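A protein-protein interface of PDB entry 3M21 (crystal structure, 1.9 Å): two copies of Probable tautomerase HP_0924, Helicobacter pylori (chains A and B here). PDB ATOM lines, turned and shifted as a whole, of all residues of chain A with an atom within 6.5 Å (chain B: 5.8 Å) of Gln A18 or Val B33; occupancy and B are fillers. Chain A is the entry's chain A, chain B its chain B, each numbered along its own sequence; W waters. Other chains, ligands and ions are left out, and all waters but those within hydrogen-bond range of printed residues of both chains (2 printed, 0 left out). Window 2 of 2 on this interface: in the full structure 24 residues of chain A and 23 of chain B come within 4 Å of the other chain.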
ATOM      1  N   GLU A  10      -6.997   1.157 -21.149  1.00  0.00           N
ATOM      2  CA  GLU A  10      -6.772   0.159 -22.180  1.00  0.00           C
ATOM      3  C   GLU A  10      -7.465   0.568 -23.475  1.00  0.00           C
ATOM      4  O   GLU A  10      -8.565   1.131 -23.464  1.00  0.00           O
ATOM      5  CB  GLU A  10      -7.274  -1.217 -21.723  1.00  0.00           C
ATOM      6  CG  GLU A  10      -8.787  -1.358 -21.630  1.00  0.00           C
ATOM      7  CD  GLU A  10      -9.222  -2.796 -21.334  1.00  0.00           C
ATOM      8  OE1 GLU A  10      -8.502  -3.740 -21.743  1.00  0.00           O
ATOM      9  OE2 GLU A  10     -10.289  -2.982 -20.708  1.00  0.00           O
ATOM     10  N   ASN A  11      -6.798   0.288 -24.590  1.00  0.00           N
ATOM     11  CA  ASN A  11      -7.323   0.608 -25.909  1.00  0.00           C
ATOM     12  C   ASN A  11      -7.598   2.103 -26.057  1.00  0.00           C
ATOM     13  O   ASN A  11      -8.653   2.514 -26.550  1.00  0.00           O
ATOM     14  CB  ASN A  11      -8.598  -0.195 -26.163  1.00  0.00           C
ATOM     15  CG  ASN A  11      -9.109  -0.037 -27.579  1.00  0.00           C
ATOM     16  OD1 ASN A  11      -8.341  -0.138 -28.540  1.00  0.00           O
ATOM     17  ND2 ASN A  11     -10.411   0.202 -27.719  1.00  0.00           N
ATOM     18  N   GLY A  12      -6.638   2.914 -25.620  1.00  0.00           N
ATOM     19  CA  GLY A  12      -6.777   4.355 -25.712  1.00  0.00           C
ATOM     20  C   GLY A  12      -7.849   4.930 -24.799  1.00  0.00           C
ATOM     21  O   GLY A  12      -8.001   6.147 -24.727  1.00  0.00           O
ATOM     22  N   GLY A  13      -8.583   4.068 -24.098  1.00  0.00           N
ATOM     23  CA  GLY A  13      -9.635   4.541 -23.211  1.00  0.00           C
ATOM     24  C   GLY A  13      -9.339   4.384 -21.726  1.00  0.00           C
ATOM     25  O   GLY A  13      -8.264   3.911 -21.356  1.00  0.00           O
ATOM     26  N   PRO A  14     -10.272   4.782 -20.842  1.00  0.00           N
ATOM     27  CA  PRO A  14     -11.580   5.370 -21.151  1.00  0.00           C
ATOM     28  C   PRO A  14     -11.461   6.806 -21.653  1.00  0.00           C
ATOM     29  O   PRO A  14     -10.687   7.598 -21.122  1.00  0.00           O
ATOM     30  CB  PRO A  14     -12.307   5.303 -19.814  1.00  0.00           C
ATOM     31  CG  PRO A  14     -11.201   5.558 -18.849  1.00  0.00           C
ATOM     32  CD  PRO A  14     -10.088   4.678 -19.383  1.00  0.00           C
ATOM     33  N   THR A  15     -12.231   7.129 -22.685  1.00  0.00           N
ATOM     34  CA  THR A  15     -12.234   8.468 -23.258  1.00  0.00           C
ATOM     35  C   THR A  15     -12.958   9.384 -22.292  1.00  0.00           C
ATOM     36  O   THR A  15     -13.600   8.916 -21.352  1.00  0.00           O
ATOM     37  CB  THR A  15     -12.999   8.500 -24.591  1.00  0.00           C
ATOM     38  OG1 THR A  15     -14.379   8.182 -24.355  1.00  0.00           O
ATOM     39  CG2 THR A  15     -12.409   7.493 -25.552  1.00  0.00           C
ATOM     40  N   ASN A  16     -12.863  10.687 -22.533  1.00  0.00           N
ATOM     41  CA  ASN A  16     -13.541  11.652 -21.675  1.00  0.00           C
ATOM     42  C   ASN A  16     -15.047  11.459 -21.742  1.00  0.00           C
ATOM     43  O   ASN A  16     -15.761  11.762 -20.782  1.00  0.00           O
ATOM     44  CB  ASN A  16     -13.199  13.086 -22.074  1.00  0.00           C
ATOM     45  CG  ASN A  16     -11.740  13.422 -21.836  1.00  0.00           C
ATOM     46  OD1 ASN A  16     -11.137  12.975 -20.855  1.00  0.00           O
ATOM     47  ND2 ASN A  16     -11.167  14.226 -22.722  1.00  0.00           N
ATOM     48  N   GLU A  17     -15.536  10.954 -22.873  1.00  0.00           N
ATOM     49  CA  GLU A  17     -16.963  10.734 -23.009  1.00  0.00           C
ATOM     50  C   GLU A  17     -17.387   9.546 -22.156  1.00  0.00           C
ATOM     51  O   GLU A  17     -18.425   9.589 -21.494  1.00  0.00           O
ATOM     52  CB  GLU A  17     -17.345  10.494 -24.472  1.00  0.00           C
ATOM     53  CG  GLU A  17     -18.857  10.400 -24.672  1.00  0.00           C
ATOM     54  CD  GLU A  17     -19.271  10.483 -26.132  1.00  0.00           C
ATOM     55  OE1 GLU A  17     -18.947   9.550 -26.899  1.00  0.00           O
ATOM     56  OE2 GLU A  17     -19.914  11.493 -26.514  1.00  0.00           O
ATOM     57  N   GLN A  18     -16.584   8.488 -22.176  1.00  0.00           N
ATOM     58  CA  GLN A  18     -16.886   7.297 -21.387  1.00  0.00           C
ATOM     59  C   GLN A  18     -16.828   7.671 -19.906  1.00  0.00           C
ATOM     60  O   GLN A  18     -17.623   7.185 -19.104  1.00  0.00           O
ATOM     61  CB  GLN A  18     -15.886   6.181 -21.683  1.00  0.00           C
ATOM     62  CG  GLN A  18     -15.963   5.639 -23.111  1.00  0.00           C
ATOM     63  CD  GLN A  18     -14.907   4.593 -23.397  1.00  0.00           C
ATOM     64  OE1 GLN A  18     -13.711   4.854 -23.271  1.00  0.00           O
ATOM     65  NE2 GLN A  18     -15.343   3.400 -23.785  1.00  0.00           N
ATOM     66  N   LYS A  19     -15.883   8.537 -19.548  1.00  0.00           N
ATOM     67  CA  LYS A  19     -15.762   8.971 -18.166  1.00  0.00           C
ATOM     68  C   LYS A  19     -17.034   9.719 -17.774  1.00  0.00           C
ATOM     69  O   LYS A  19     -17.547   9.551 -16.666  1.00  0.00           O
ATOM     70  CB  LYS A  19     -14.535   9.873 -17.984  1.00  0.00           C
ATOM     71  CG  LYS A  19     -13.180   9.182 -18.166  1.00  0.00           C
ATOM     72  CD  LYS A  19     -12.044  10.194 -18.038  1.00  0.00           C
ATOM     73  CE  LYS A  19     -10.683   9.598 -18.342  1.00  0.00           C
ATOM     74  NZ  LYS A  19      -9.639  10.665 -18.330  1.00  0.00           N
ATOM     75  N   GLN A  20     -17.549  10.541 -18.685  1.00  0.00           N
ATOM     76  CA  GLN A  20     -18.776  11.297 -18.411  1.00  0.00           C
ATOM     77  C   GLN A  20     -19.936  10.331 -18.189  1.00  0.00           C
ATOM     78  O   GLN A  20     -20.775  10.533 -17.304  1.00  0.00           O
ATOM     79  CB  GLN A  20     -19.104  12.235 -19.585  1.00  0.00           C
ATOM     80  CG  GLN A  20     -18.104  13.366 -19.778  1.00  0.00           C
ATOM     81  CD  GLN A  20     -18.330  14.143 -21.064  1.00  0.00           C
ATOM     82  OE1 GLN A  20     -19.442  14.594 -21.343  1.00  0.00           O
ATOM     83  NE2 GLN A  20     -17.269  14.312 -21.849  1.00  0.00           N
ATOM     84  N   GLN A  21     -19.976   9.278 -18.997  1.00  0.00           N
ATOM     85  CA  GLN A  21     -21.034   8.275 -18.883  1.00  0.00           C
ATOM     86  C   GLN A  21     -20.944   7.541 -17.540  1.00  0.00           C
ATOM     87  O   GLN A  21     -21.965   7.171 -16.958  1.00  0.00           O
ATOM     88  CB  GLN A  21     -20.954   7.278 -20.043  1.00  0.00           C
ATOM     89  CG  GLN A  21     -21.073   7.942 -21.412  1.00  0.00           C
ATOM     90  CD  GLN A  21     -21.150   6.945 -22.557  1.00  0.00           C
ATOM     91  OE1 GLN A  21     -20.271   6.093 -22.720  1.00  0.00           O
ATOM     92  NE2 GLN A  21     -22.205   7.055 -23.368  1.00  0.00           N
ATOM     93  N   LEU A  22     -19.726   7.337 -17.044  1.00  0.00           N
ATOM     94  CA  LEU A  22     -19.569   6.671 -15.756  1.00  0.00           C
ATOM     95  C   LEU A  22     -20.078   7.557 -14.624  1.00  0.00           C
ATOM     96  O   LEU A  22     -20.814   7.090 -13.748  1.00  0.00           O
ATOM     97  CB  LEU A  22     -18.104   6.287 -15.506  1.00  0.00           C
ATOM     98  CG  LEU A  22     -17.517   5.143 -16.343  1.00  0.00           C
ATOM     99  CD1 LEU A  22     -16.097   4.833 -15.849  1.00  0.00           C
ATOM    100  CD2 LEU A  22     -18.394   3.896 -16.229  1.00  0.00           C
ATOM    101  N   ILE A  23     -19.692   8.833 -14.640  1.00  0.00           N
ATOM    102  CA  ILE A  23     -20.126   9.775 -13.608  1.00  0.00           C
ATOM    103  C   ILE A  23     -21.652   9.876 -13.593  1.00  0.00           C
ATOM    104  O   ILE A  23     -22.276   9.827 -12.531  1.00  0.00           O
ATOM    105  CB  ILE A  23     -19.507  11.187 -13.831  1.00  0.00           C
ATOM    106  CG1 ILE A  23     -17.986  11.123 -13.623  1.00  0.00           C
ATOM    107  CG2 ILE A  23     -20.122  12.193 -12.860  1.00  0.00           C
ATOM    108  CD1 ILE A  23     -17.261  12.409 -13.910  1.00  0.00           C
ATOM    109  N   ILE A  45     -12.675   9.192 -10.601  1.00  0.00           N
ATOM    110  CA  ILE A  45     -12.191   8.048 -11.347  1.00  0.00           C
ATOM    111  C   ILE A  45     -10.669   8.112 -11.345  1.00  0.00           C
ATOM    112  O   ILE A  45     -10.081   9.115 -11.766  1.00  0.00           O
ATOM    113  CB  ILE A  45     -12.689   8.109 -12.807  1.00  0.00           C
ATOM    114  CG1 ILE A  45     -14.215   8.137 -12.826  1.00  0.00           C
ATOM    115  CG2 ILE A  45     -12.166   6.926 -13.592  1.00  0.00           C
ATOM    116  CD1 ILE A  45     -14.801   8.582 -14.136  1.00  0.00           C
ATOM    117  N   ASP B  28     -22.618  -3.619 -13.614  1.00  0.00           N
ATOM    118  CA  ASP B  28     -23.177  -3.640 -14.964  1.00  0.00           C
ATOM    119  C   ASP B  28     -22.819  -2.366 -15.729  1.00  0.00           C
ATOM    120  O   ASP B  28     -22.698  -2.385 -16.957  1.00  0.00           O
ATOM    121  CB  ASP B  28     -24.703  -3.804 -14.930  1.00  0.00           C
ATOM    122  CG  ASP B  28     -25.137  -5.157 -14.388  1.00  0.00           C
ATOM    123  OD1 ASP B  28     -24.510  -6.180 -14.748  1.00  0.00           O
ATOM    124  OD2 ASP B  28     -26.118  -5.196 -13.616  1.00  0.00           O
ATOM    125  N   LEU B  29     -22.657  -1.259 -15.009  1.00  0.00           N
ATOM    126  CA  LEU B  29     -22.308   0.007 -15.651  1.00  0.00           C
ATOM    127  C   LEU B  29     -20.931  -0.105 -16.293  1.00  0.00           C
ATOM    128  O   LEU B  29     -20.738   0.292 -17.447  1.00  0.00           O
ATOM    129  CB  LEU B  29     -22.312   1.148 -14.631  1.00  0.00           C
ATOM    130  CG  LEU B  29     -22.046   2.553 -15.182  1.00  0.00           C
ATOM    131  CD1 LEU B  29     -23.112   2.929 -16.213  1.00  0.00           C
ATOM    132  CD2 LEU B  29     -22.037   3.550 -14.041  1.00  0.00           C
ATOM    133  N   MET B  30     -19.982  -0.652 -15.538  1.00  0.00           N
ATOM    134  CA  MET B  30     -18.614  -0.837 -16.011  1.00  0.00           C
ATOM    135  C   MET B  30     -18.597  -1.687 -17.277  1.00  0.00           C
ATOM    136  O   MET B  30     -17.856  -1.401 -18.219  1.00  0.00           O
ATOM    137  CB  MET B  30     -17.765  -1.520 -14.936  1.00  0.00           C
ATOM    138  CG  MET B  30     -17.625  -0.748 -13.634  1.00  0.00           C
ATOM    139  SD  MET B  30     -16.763   0.814 -13.800  1.00  0.00           S
ATOM    140  CE  MET B  30     -18.135   1.930 -13.721  1.00  0.00           C
ATOM    141  N   VAL B  31     -19.408  -2.742 -17.291  1.00  0.00           N
ATOM    142  CA  VAL B  31     -19.478  -3.621 -18.450  1.00  0.00           C
ATOM    143  C   VAL B  31     -20.097  -2.907 -19.652  1.00  0.00           C
ATOM    144  O   VAL B  31     -19.612  -3.041 -20.776  1.00  0.00           O
ATOM    145  CB  VAL B  31     -20.285  -4.879 -18.108  1.00  0.00           C
ATOM    146  N   LYS B  32     -21.156  -2.142 -19.413  1.00  0.00           N
ATOM    147  CA  LYS B  32     -21.840  -1.423 -20.486  1.00  0.00           C
ATOM    148  C   LYS B  32     -21.052  -0.257 -21.066  1.00  0.00           C
ATOM    149  O   LYS B  32     -21.029  -0.063 -22.279  1.00  0.00           O
ATOM    150  CB  LYS B  32     -23.196  -0.900 -20.003  1.00  0.00           C
ATOM    151  CG  LYS B  32     -23.910  -0.013 -21.023  1.00  0.00           C
ATOM    152  CD  LYS B  32     -25.356   0.249 -20.630  1.00  0.00           C
ATOM    153  CE  LYS B  32     -26.089   1.040 -21.706  1.00  0.00           C
ATOM    154  NZ  LYS B  32     -27.533   1.216 -21.367  1.00  0.00           N
ATOM    155  N   VAL B  33     -20.411   0.520 -20.201  1.00  0.00           N
ATOM    156  CA  VAL B  33     -19.657   1.673 -20.658  1.00  0.00           C
ATOM    157  C   VAL B  33     -18.245   1.354 -21.134  1.00  0.00           C
ATOM    158  O   VAL B  33     -17.788   1.904 -22.136  1.00  0.00           O
ATOM    159  CB  VAL B  33     -19.570   2.744 -19.558  1.00  0.00           C
ATOM    160  CG1 VAL B  33     -18.863   3.980 -20.092  1.00  0.00           C
ATOM    161  CG2 VAL B  33     -20.964   3.095 -19.064  1.00  0.00           C
ATOM    162  N   LEU B  34     -17.555   0.465 -20.427  1.00  0.00           N
ATOM    163  CA  LEU B  34     -16.183   0.120 -20.786  1.00  0.00           C
ATOM    164  C   LEU B  34     -15.981  -1.328 -21.198  1.00  0.00           C
ATOM    165  O   LEU B  34     -14.863  -1.738 -21.509  1.00  0.00           O
ATOM    166  CB  LEU B  34     -15.243   0.446 -19.622  1.00  0.00           C
ATOM    167  CG  LEU B  34     -15.142   1.925 -19.246  1.00  0.00           C
ATOM    168  CD1 LEU B  34     -14.286   2.084 -18.008  1.00  0.00           C
ATOM    169  CD2 LEU B  34     -14.549   2.702 -20.416  1.00  0.00           C
ATOM    170  N   ASN B  35     -17.057  -2.106 -21.205  1.00  0.00           N
ATOM    171  CA  ASN B  35     -16.960  -3.511 -21.578  1.00  0.00           C
ATOM    172  C   ASN B  35     -15.940  -4.212 -20.683  1.00  0.00           C
ATOM    173  O   ASN B  35     -15.215  -5.105 -21.126  1.00  0.00           O
ATOM    174  CB  ASN B  35     -16.542  -3.633 -23.048  1.00  0.00           C
ATOM    175  CG  ASN B  35     -17.464  -2.867 -23.982  1.00  0.00           C
ATOM    176  OD1 ASN B  35     -18.643  -3.193 -24.112  1.00  0.00           O
ATOM    177  ND2 ASN B  35     -16.929  -1.837 -24.630  1.00  0.00           N
HETATM  178  O   HOH W   1     -12.315  -1.266 -21.409  1.00  0.00           O
HETATM  179  O   HOH W   2     -19.508   3.698 -23.996  1.00  0.00           O
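No position is printed for both chains.
Pro A14 touches Leu B34. Leu B34 touches Gln A18 (CD2 to NE2, 3.5 Å). Val B33 touches Gln A21. Leu A22 touches Leu B29. Leu A22 touches Met B30 (CD2 to CE, 3.2 Å). Val B33 touches Leu A22. Leu A22 touches Leu B34 (CD1 to CD1, 3.9 Å).
Water W1 bridges O of Leu B34 and OE2 of Glu A10. Water W2 bridges the side-chain amide oxygen (OE1) of Gln A21 (2.8 Å) and the backbone carbonyl oxygen (O) of Val B33 (3.1 Å).
Hydrophobic or aromatic side chains of chain A within 4 Å of the printed part of chain B: Pro A14 and Leu A22. Along chain A the printed residues that touch a printed residue of chain B span positions 14 to 22. Of the 8 printed residues of chain B, 4 touch a printed residue of chain A. Hydrophobic or aromatic side chains of chain B that line the printed part of chain A: Leu B29, Met B30, Val B33 and Leu B34. Among the printed residues, 8 pairs touch across the chains. Among the printed residues, no Asp or Glu carboxylate lies within 4 Å of a Lys or Arg side-chain nitrogen of the other chain.
Gln A18 touches two residues of chain B. Of the printed residues of chain A, Met B30 touches Leu A22. Of the printed residues of chain B, Pro A14 touches Leu B34. Printed residues of chain A within 4 Å of Leu B29: Leu A22 (3.8 Å). Asn A11 touches none of the printed residues of chain B. The nearest residue of chain B that does not touch Gln A18 is Asn B35 (5.5 Å). The nearest printed residue of chain A that does not touch Leu B34 is Glu A10 (4.8 Å).
The side-chain amide nitrogen of Gln A18 is in hydrogen-bond range of the backbone carbonyl oxygen of Val B33 (3.3 Å).
N of Thr A15 lies within hydrogen-bond range of OE1 of Gln A18 (2.8 Å). O of Met B30 lies within hydrogen-bond range of N of Asn B35 (3.2 Å).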
